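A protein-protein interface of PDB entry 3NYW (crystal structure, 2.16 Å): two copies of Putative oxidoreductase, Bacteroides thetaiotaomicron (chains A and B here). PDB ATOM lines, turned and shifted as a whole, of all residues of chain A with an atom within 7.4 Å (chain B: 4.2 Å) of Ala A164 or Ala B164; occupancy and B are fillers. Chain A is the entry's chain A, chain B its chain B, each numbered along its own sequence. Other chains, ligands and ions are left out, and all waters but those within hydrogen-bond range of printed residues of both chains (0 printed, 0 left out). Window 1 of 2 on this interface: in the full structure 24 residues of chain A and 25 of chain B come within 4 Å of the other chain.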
ATOM      1  N   PHE A 110     -27.494 -16.573  19.800  1.00  0.00           N
ATOM      2  CA  PHE A 110     -26.211 -16.804  20.447  1.00  0.00           C
ATOM      3  C   PHE A 110     -26.447 -17.555  21.758  1.00  0.00           C
ATOM      4  O   PHE A 110     -25.704 -18.469  22.094  1.00  0.00           O
ATOM      5  CB  PHE A 110     -25.488 -15.471  20.698  1.00  0.00           C
ATOM      6  CG  PHE A 110     -24.052 -15.626  21.146  1.00  0.00           C
ATOM      7  CD1 PHE A 110     -23.261 -16.662  20.655  1.00  0.00           C
ATOM      8  CD2 PHE A 110     -23.486 -14.727  22.042  1.00  0.00           C
ATOM      9  CE1 PHE A 110     -21.925 -16.801  21.054  1.00  0.00           C
ATOM     10  CE2 PHE A 110     -22.155 -14.857  22.444  1.00  0.00           C
ATOM     11  CZ  PHE A 110     -21.375 -15.900  21.947  1.00  0.00           C
ATOM     12  N   MET A 114     -24.972 -21.273  22.451  1.00  0.00           N
ATOM     13  CA  MET A 114     -24.087 -21.493  23.589  1.00  0.00           C
ATOM     14  C   MET A 114     -24.662 -22.589  24.499  1.00  0.00           C
ATOM     15  O   MET A 114     -23.933 -23.440  25.010  1.00  0.00           O
ATOM     16  CB  MET A 114     -23.925 -20.183  24.369  1.00  0.00           C
ATOM     17  CG  MET A 114     -22.835 -20.191  25.431  1.00  0.00           C
ATOM     18  SD  MET A 114     -21.050 -20.470  24.697  1.00  0.00           S
ATOM     19  CE  MET A 114     -21.235 -19.524  23.012  1.00  0.00           C
ATOM     20  N   ASN A 117     -24.298 -26.163  22.710  1.00  0.00           N
ATOM     21  CA  ASN A 117     -22.930 -26.644  22.512  1.00  0.00           C
ATOM     22  C   ASN A 117     -21.981 -26.595  23.699  1.00  0.00           C
ATOM     23  O   ASN A 117     -21.148 -27.484  23.850  1.00  0.00           O
ATOM     24  CB  ASN A 117     -22.268 -25.899  21.358  1.00  0.00           C
ATOM     25  CG  ASN A 117     -23.107 -25.919  20.113  1.00  0.00           C
ATOM     26  OD1 ASN A 117     -23.792 -24.945  19.793  1.00  0.00           O
ATOM     27  ND2 ASN A 117     -23.078 -27.038  19.410  1.00  0.00           N
ATOM     28  N   VAL A 118     -22.083 -25.564  24.530  1.00  0.00           N
ATOM     29  CA  VAL A 118     -21.172 -25.452  25.661  1.00  0.00           C
ATOM     30  C   VAL A 118     -21.749 -25.861  27.009  1.00  0.00           C
ATOM     31  O   VAL A 118     -21.149 -26.665  27.720  1.00  0.00           O
ATOM     32  CB  VAL A 118     -20.613 -24.035  25.764  1.00  0.00           C
ATOM     33  CG1 VAL A 118     -19.532 -23.984  26.834  1.00  0.00           C
ATOM     34  CG2 VAL A 118     -20.054 -23.615  24.416  1.00  0.00           C
ATOM     35  N   GLY A 156     -18.995 -13.180  15.280  1.00  0.00           N
ATOM     36  CA  GLY A 156     -18.218 -13.809  16.330  1.00  0.00           C
ATOM     37  C   GLY A 156     -18.877 -14.986  17.025  1.00  0.00           C
ATOM     38  O   GLY A 156     -18.266 -15.604  17.893  1.00  0.00           O
ATOM     39  N   TYR A 158     -19.683 -18.143  15.956  1.00  0.00           N
ATOM     40  CA  TYR A 158     -19.043 -19.441  15.779  1.00  0.00           C
ATOM     41  C   TYR A 158     -17.735 -19.508  16.563  1.00  0.00           C
ATOM     42  O   TYR A 158     -17.567 -20.361  17.424  1.00  0.00           O
ATOM     43  CB  TYR A 158     -18.752 -19.722  14.301  1.00  0.00           C
ATOM     44  CG  TYR A 158     -18.171 -21.100  14.068  1.00  0.00           C
ATOM     45  CD1 TYR A 158     -18.972 -22.238  14.151  1.00  0.00           C
ATOM     46  CD2 TYR A 158     -16.806 -21.270  13.819  1.00  0.00           C
ATOM     47  CE1 TYR A 158     -18.430 -23.515  13.999  1.00  0.00           C
ATOM     48  CE2 TYR A 158     -16.251 -22.546  13.664  1.00  0.00           C
ATOM     49  CZ  TYR A 158     -17.069 -23.661  13.756  1.00  0.00           C
ATOM     50  OH  TYR A 158     -16.529 -24.921  13.607  1.00  0.00           O
ATOM     51  N   GLY A 159     -16.813 -18.602  16.256  1.00  0.00           N
ATOM     52  CA  GLY A 159     -15.525 -18.589  16.932  1.00  0.00           C
ATOM     53  C   GLY A 159     -15.593 -18.626  18.447  1.00  0.00           C
ATOM     54  O   GLY A 159     -14.805 -19.311  19.095  1.00  0.00           O
ATOM     55  N   SER A 160     -16.539 -17.890  19.015  1.00  0.00           N
ATOM     56  CA  SER A 160     -16.703 -17.835  20.459  1.00  0.00           C
ATOM     57  C   SER A 160     -17.108 -19.196  21.047  1.00  0.00           C
ATOM     58  O   SER A 160     -16.563 -19.633  22.067  1.00  0.00           O
ATOM     59  CB  SER A 160     -17.751 -16.779  20.809  1.00  0.00           C
ATOM     60  OG  SER A 160     -17.903 -16.662  22.209  1.00  0.00           O
ATOM     61  N   THR A 161     -18.067 -19.858  20.401  1.00  0.00           N
ATOM     62  CA  THR A 161     -18.545 -21.161  20.853  1.00  0.00           C
ATOM     63  C   THR A 161     -17.433 -22.212  20.749  1.00  0.00           C
ATOM     64  O   THR A 161     -17.282 -23.067  21.619  1.00  0.00           O
ATOM     65  CB  THR A 161     -19.762 -21.620  20.020  1.00  0.00           C
ATOM     66  OG1 THR A 161     -20.774 -20.602  20.049  1.00  0.00           O
ATOM     67  CG2 THR A 161     -20.342 -22.902  20.587  1.00  0.00           C
ATOM     68  N   LYS A 162     -16.650 -22.129  19.682  1.00  0.00           N
ATOM     69  CA  LYS A 162     -15.548 -23.048  19.464  1.00  0.00           C
ATOM     70  C   LYS A 162     -14.481 -22.900  20.559  1.00  0.00           C
ATOM     71  O   LYS A 162     -14.063 -23.887  21.160  1.00  0.00           O
ATOM     72  CB  LYS A 162     -14.924 -22.789  18.093  1.00  0.00           C
ATOM     73  CG  LYS A 162     -14.007 -23.898  17.609  1.00  0.00           C
ATOM     74  CD  LYS A 162     -13.485 -23.592  16.191  1.00  0.00           C
ATOM     75  CE  LYS A 162     -12.638 -24.749  15.642  1.00  0.00           C
ATOM     76  NZ  LYS A 162     -11.401 -24.961  16.451  1.00  0.00           N
ATOM     77  N   PHE A 163     -14.041 -21.675  20.824  1.00  0.00           N
ATOM     78  CA  PHE A 163     -13.032 -21.468  21.856  1.00  0.00           C
ATOM     79  C   PHE A 163     -13.544 -21.839  23.238  1.00  0.00           C
ATOM     80  O   PHE A 163     -12.812 -22.410  24.034  1.00  0.00           O
ATOM     81  CB  PHE A 163     -12.536 -20.024  21.874  1.00  0.00           C
ATOM     82  CG  PHE A 163     -11.593 -19.687  20.752  1.00  0.00           C
ATOM     83  CD1 PHE A 163     -10.536 -18.807  20.963  1.00  0.00           C
ATOM     84  CD2 PHE A 163     -11.785 -20.208  19.478  1.00  0.00           C
ATOM     85  CE1 PHE A 163      -9.681 -18.446  19.919  1.00  0.00           C
ATOM     86  CE2 PHE A 163     -10.935 -19.853  18.425  1.00  0.00           C
ATOM     87  CZ  PHE A 163      -9.883 -18.970  18.646  1.00  0.00           C
ATOM     88  N   ALA A 164     -14.798 -21.508  23.525  1.00  0.00           N
ATOM     89  CA  ALA A 164     -15.376 -21.839  24.819  1.00  0.00           C
ATOM     90  C   ALA A 164     -15.175 -23.329  25.086  1.00  0.00           C
ATOM     91  O   ALA A 164     -14.876 -23.734  26.204  1.00  0.00           O
ATOM     92  CB  ALA A 164     -16.852 -21.499  24.835  1.00  0.00           C
ATOM     93  N   LEU A 165     -15.344 -24.148  24.056  1.00  0.00           N
ATOM     94  CA  LEU A 165     -15.156 -25.581  24.218  1.00  0.00           C
ATOM     95  C   LEU A 165     -13.681 -25.900  24.467  1.00  0.00           C
ATOM     96  O   LEU A 165     -13.353 -26.692  25.337  1.00  0.00           O
ATOM     97  CB  LEU A 165     -15.669 -26.321  22.984  1.00  0.00           C
ATOM     98  CG  LEU A 165     -17.195 -26.359  22.906  1.00  0.00           C
ATOM     99  CD1 LEU A 165     -17.640 -26.728  21.497  1.00  0.00           C
ATOM    100  CD2 LEU A 165     -17.729 -27.346  23.940  1.00  0.00           C
ATOM    101  N   LEU A 166     -12.792 -25.271  23.705  1.00  0.00           N
ATOM    102  CA  LEU A 166     -11.360 -25.486  23.876  1.00  0.00           C
ATOM    103  C   LEU A 166     -10.907 -25.016  25.264  1.00  0.00           C
ATOM    104  O   LEU A 166     -10.046 -25.639  25.898  1.00  0.00           O
ATOM    105  CB  LEU A 166     -10.584 -24.730  22.799  1.00  0.00           C
ATOM    106  CG  LEU A 166     -10.753 -25.224  21.357  1.00  0.00           C
ATOM    107  CD1 LEU A 166      -9.849 -24.403  20.426  1.00  0.00           C
ATOM    108  CD2 LEU A 166     -10.396 -26.716  21.270  1.00  0.00           C
ATOM    109  N   GLY A 167     -11.490 -23.913  25.727  1.00  0.00           N
ATOM    110  CA  GLY A 167     -11.142 -23.389  27.031  1.00  0.00           C
ATOM    111  C   GLY A 167     -11.537 -24.360  28.122  1.00  0.00           C
ATOM    112  O   GLY A 167     -10.841 -24.519  29.120  1.00  0.00           O
ATOM    113  N   LEU A 168     -12.665 -25.019  27.922  1.00  0.00           N
ATOM    114  CA  LEU A 168     -13.163 -25.982  28.878  1.00  0.00           C
ATOM    115  C   LEU A 168     -12.208 -27.190  28.928  1.00  0.00           C
ATOM    116  O   LEU A 168     -11.775 -27.625  30.007  1.00  0.00           O
ATOM    117  CB  LEU A 168     -14.564 -26.400  28.452  1.00  0.00           C
ATOM    118  CG  LEU A 168     -15.469 -27.130  29.435  1.00  0.00           C
ATOM    119  CD1 LEU A 168     -15.550 -26.365  30.743  1.00  0.00           C
ATOM    120  CD2 LEU A 168     -16.848 -27.268  28.799  1.00  0.00           C
ATOM    121  N   ALA A 169     -11.861 -27.703  27.751  1.00  0.00           N
ATOM    122  CA  ALA A 169     -10.953 -28.839  27.632  1.00  0.00           C
ATOM    123  C   ALA A 169      -9.592 -28.535  28.277  1.00  0.00           C
ATOM    124  O   ALA A 169      -9.078 -29.307  29.077  1.00  0.00           O
ATOM    125  CB  ALA A 169     -10.759 -29.195  26.156  1.00  0.00           C
ATOM    126  N   GLU A 170      -9.021 -27.396  27.929  1.00  0.00           N
ATOM    127  CA  GLU A 170      -7.723 -27.025  28.462  1.00  0.00           C
ATOM    128  C   GLU A 170      -7.687 -27.004  29.985  1.00  0.00           C
ATOM    129  O   GLU A 170      -6.729 -27.482  30.582  1.00  0.00           O
ATOM    130  CB  GLU A 170      -7.295 -25.669  27.900  1.00  0.00           C
ATOM    131  CG  GLU A 170      -5.797 -25.420  27.974  1.00  0.00           C
ATOM    132  CD  GLU A 170      -5.279 -24.652  26.767  1.00  0.00           C
ATOM    133  OE1 GLU A 170      -5.642 -25.020  25.624  1.00  0.00           O
ATOM    134  OE2 GLU A 170      -4.501 -23.693  26.960  1.00  0.00           O
ATOM    135  N   SER A 171      -8.720 -26.465  30.622  1.00  0.00           N
ATOM    136  CA  SER A 171      -8.710 -26.428  32.077  1.00  0.00           C
ATOM    137  C   SER A 171      -8.922 -27.807  32.698  1.00  0.00           C
ATOM    138  O   SER A 171      -8.308 -28.120  33.709  1.00  0.00           O
ATOM    139  CB  SER A 171      -9.736 -25.413  32.624  1.00  0.00           C
ATOM    140  OG  SER A 171     -11.050 -25.665  32.167  1.00  0.00           O
ATOM    141  N   VAL B 118     -20.257 -13.277  28.478  1.00  0.00           N
ATOM    142  CA  VAL B 118     -20.121 -13.408  27.033  1.00  0.00           C
ATOM    143  C   VAL B 118     -21.347 -12.978  26.238  1.00  0.00           C
ATOM    144  O   VAL B 118     -21.221 -12.253  25.255  1.00  0.00           O
ATOM    145  CB  VAL B 118     -19.759 -14.859  26.654  1.00  0.00           C
ATOM    146  CG1 VAL B 118     -19.522 -14.968  25.165  1.00  0.00           C
ATOM    147  CG2 VAL B 118     -18.526 -15.293  27.424  1.00  0.00           C
ATOM    148  N   SER B 160     -13.424 -21.563  30.247  1.00  0.00           N
ATOM    149  CA  SER B 160     -14.335 -21.552  29.116  1.00  0.00           C
ATOM    150  C   SER B 160     -14.755 -20.114  28.786  1.00  0.00           C
ATOM    151  O   SER B 160     -14.615 -19.659  27.648  1.00  0.00           O
ATOM    152  CB  SER B 160     -15.566 -22.406  29.427  1.00  0.00           C
ATOM    153  OG  SER B 160     -16.375 -22.565  28.276  1.00  0.00           O
ATOM    154  N   THR B 161     -15.257 -19.402  29.788  1.00  0.00           N
ATOM    155  CA  THR B 161     -15.687 -18.019  29.601  1.00  0.00           C
ATOM    156  C   THR B 161     -14.579 -17.163  28.982  1.00  0.00           C
ATOM    157  O   THR B 161     -14.796 -16.466  27.993  1.00  0.00           O
ATOM    158  CB  THR B 161     -16.102 -17.377  30.937  1.00  0.00           C
ATOM    159  OG1 THR B 161     -17.028 -18.238  31.615  1.00  0.00           O
ATOM    160  CG2 THR B 161     -16.766 -16.023  30.693  1.00  0.00           C
ATOM    161  N   LYS B 162     -13.389 -17.234  29.564  1.00  0.00           N
ATOM    162  CA  LYS B 162     -12.260 -16.454  29.086  1.00  0.00           C
ATOM    163  C   LYS B 162     -11.956 -16.728  27.620  1.00  0.00           C
ATOM    164  O   LYS B 162     -11.723 -15.802  26.847  1.00  0.00           O
ATOM    165  CB  LYS B 162     -11.022 -16.741  29.936  1.00  0.00           C
ATOM    166  CG  LYS B 162      -9.977 -15.645  29.860  1.00  0.00           C
ATOM    167  CD  LYS B 162      -8.790 -15.942  30.758  1.00  0.00           C
ATOM    168  CE  LYS B 162      -7.970 -17.093  30.208  1.00  0.00           C
ATOM    169  NZ  LYS B 162      -7.404 -16.758  28.865  1.00  0.00           N
ATOM    170  N   PHE B 163     -11.951 -18.001  27.241  1.00  0.00           N
ATOM    171  CA  PHE B 163     -11.684 -18.372  25.860  1.00  0.00           C
ATOM    172  C   PHE B 163     -12.814 -17.922  24.953  1.00  0.00           C
ATOM    173  O   PHE B 163     -12.580 -17.506  23.820  1.00  0.00           O
ATOM    174  CB  PHE B 163     -11.500 -19.889  25.736  1.00  0.00           C
ATOM    175  CG  PHE B 163     -10.087 -20.350  25.944  1.00  0.00           C
ATOM    176  CD1 PHE B 163      -9.422 -20.098  27.140  1.00  0.00           C
ATOM    177  CD2 PHE B 163      -9.422 -21.047  24.939  1.00  0.00           C
ATOM    178  CE1 PHE B 163      -8.112 -20.534  27.335  1.00  0.00           C
ATOM    179  CE2 PHE B 163      -8.116 -21.489  25.115  1.00  0.00           C
ATOM    180  CZ  PHE B 163      -7.454 -21.233  26.321  1.00  0.00           C
ATOM    181  N   ALA B 164     -14.042 -18.013  25.447  1.00  0.00           N
ATOM    182  CA  ALA B 164     -15.199 -17.601  24.656  1.00  0.00           C
ATOM    183  C   ALA B 164     -15.014 -16.148  24.234  1.00  0.00           C
ATOM    184  O   ALA B 164     -15.179 -15.798  23.064  1.00  0.00           O
ATOM    185  CB  ALA B 164     -16.481 -17.757  25.473  1.00  0.00           C
ATOM    186  N   LEU B 165     -14.654 -15.305  25.195  1.00  0.00           N
ATOM    187  CA  LEU B 165     -14.428 -13.892  24.915  1.00  0.00           C
ATOM    188  C   LEU B 165     -13.307 -13.703  23.893  1.00  0.00           C
ATOM    189  O   LEU B 165     -13.396 -12.844  23.016  1.00  0.00           O
ATOM    190  CB  LEU B 165     -14.094 -13.160  26.217  1.00  0.00           C
ATOM    191  CG  LEU B 165     -15.279 -13.046  27.183  1.00  0.00           C
ATOM    192  CD1 LEU B 165     -14.794 -12.724  28.586  1.00  0.00           C
ATOM    193  CD2 LEU B 165     -16.241 -11.980  26.670  1.00  0.00           C
ATOM    194  N   LEU B 166     -12.257 -14.512  24.006  1.00  0.00           N
ATOM    195  CA  LEU B 166     -11.129 -14.435  23.082  1.00  0.00           C
ATOM    196  C   LEU B 166     -11.514 -14.873  21.668  1.00  0.00           C
ATOM    197  O   LEU B 166     -11.110 -14.248  20.685  1.00  0.00           O
ATOM    198  CB  LEU B 166      -9.966 -15.299  23.584  1.00  0.00           C
ATOM    199  CG  LEU B 166      -8.984 -14.620  24.539  1.00  0.00           C
ATOM    200  CD1 LEU B 166      -9.734 -14.083  25.756  1.00  0.00           C
ATOM    201  CD2 LEU B 166      -7.900 -15.612  24.953  1.00  0.00           C
ATOM    202  N   GLY B 167     -12.285 -15.951  21.570  1.00  0.00           N
ATOM    203  CA  GLY B 167     -12.710 -16.438  20.268  1.00  0.00           C
ATOM    204  C   GLY B 167     -13.558 -15.389  19.576  1.00  0.00           C
ATOM    205  O   GLY B 167     -13.507 -15.245  18.361  1.00  0.00           O
ATOM    206  N   LEU B 168     -14.326 -14.647  20.367  1.00  0.00           N
ATOM    207  CA  LEU B 168     -15.193 -13.591  19.860  1.00  0.00           C
ATOM    208  C   LEU B 168     -14.348 -12.449  19.315  1.00  0.00           C
ATOM    209  O   LEU B 168     -14.556 -11.993  18.189  1.00  0.00           O
ATOM    210  CB  LEU B 168     -16.092 -13.080  20.980  1.00  0.00           C
ATOM    211  CG  LEU B 168     -17.200 -12.082  20.642  1.00  0.00           C
ATOM    212  CD1 LEU B 168     -18.130 -12.659  19.589  1.00  0.00           C
ATOM    213  CD2 LEU B 168     -17.977 -11.771  21.917  1.00  0.00           C
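The backbone carbonyl oxygen (O) of Ala B164 is in hydrogen-bond range of the side-chain hydroxyl (OG) of Ser A160, at 3.0 Å. OG of Ser B160 sits at hydrogen-bond distance from O of Ala A164.
Phe A110 touches Val B118 (CE2 to CG1, 3.8 Å). OG of Ser B160 touches CG1 of Val A118, at 3.7 Å. Leu B168 touches Gly A156 (CD1 to O, 3.4 Å). Gly B167 touches Gly A159 (CA to O, 3.7 Å). Val B118 touches Ser A160 (CG1 to OG, 3.8 Å). Leu B168 touches Ser A160. Phe A163 touches Phe B163 (CB to O, 3.2 Å). Gly A167 touches Ser B160. Gly A167 touches Phe B163 (CA to CG, 3.4 Å). Glu A170 touches Phe B163 (OE2 to CZ, 3.9 Å).
The backbone carbonyl oxygen of Gly A167 is in hydrogen-bond range of the side-chain hydroxyl of Ser A171 (3.3 Å).
Ser A160 touches Gly B167, and with the chains exchanged Gly A167 touches Ser B160. Phe B163 touches its own counterpart, Phe A163. Phe A163 touches Gly B167, and with the chains exchanged Gly A167 touches Phe B163. Ala B164 touches its own counterpart, Ala A164. Positions printed for both chains: 118, 160, 161, 162, 163, 164, 165, 166, 167 and 168. Of the 15 pairs that touch across the chains among the printed residues, 10 have their exchanged pair printed and touching as well.
Of the 19 printed residues of chain A, 9 touch a printed residue of chain B. Printed residues of chain A that touch a printed residue of chain B: Phe A110, Val A118, Gly A156, Gly A159, Ser A160, Phe A163, Ala A164, Gly A167 and Glu A170. Hydrophobic or aromatic side chains of chain A that line the printed part of chain B: Phe A110, Val A118, Phe A163 and Ala A164. Of the 10 printed residues of chain B, 6 touch a printed residue of chain A. Hydrophobic or aromatic side chains of chain B that line the printed part of chain A: Val B118, Phe B163, Ala B164 and Leu B168. Among the printed residues, 15 pairs touch across the chains. Among the printed residues, no Asp or Glu carboxylate lies within 4 Å of a Lys or Arg side-chain nitrogen of the other chain.
Of the printed residues of chain B, Phe A163 touches Phe B163 (3.2 Å) and Gly B167 (3.3 Å). Of chain B, only Ser B160 (2.8 Å) and Ala B164 (3.8 Å) come within 4 Å of Ala A164. Printed residues of chain A within 4 Å of Phe B163: Phe A163 (3.2 Å), Gly A167 (3.4 Å) and Glu A170 (3.9 Å). Of the printed residues of chain A, Gly B167 touches Gly A159 (3.7 Å), Ser A160 (3.9 Å) and Phe A163 (3.3 Å). The nearest residue of chain A that does not touch Ala B164 is Phe A163 (4.4 Å).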
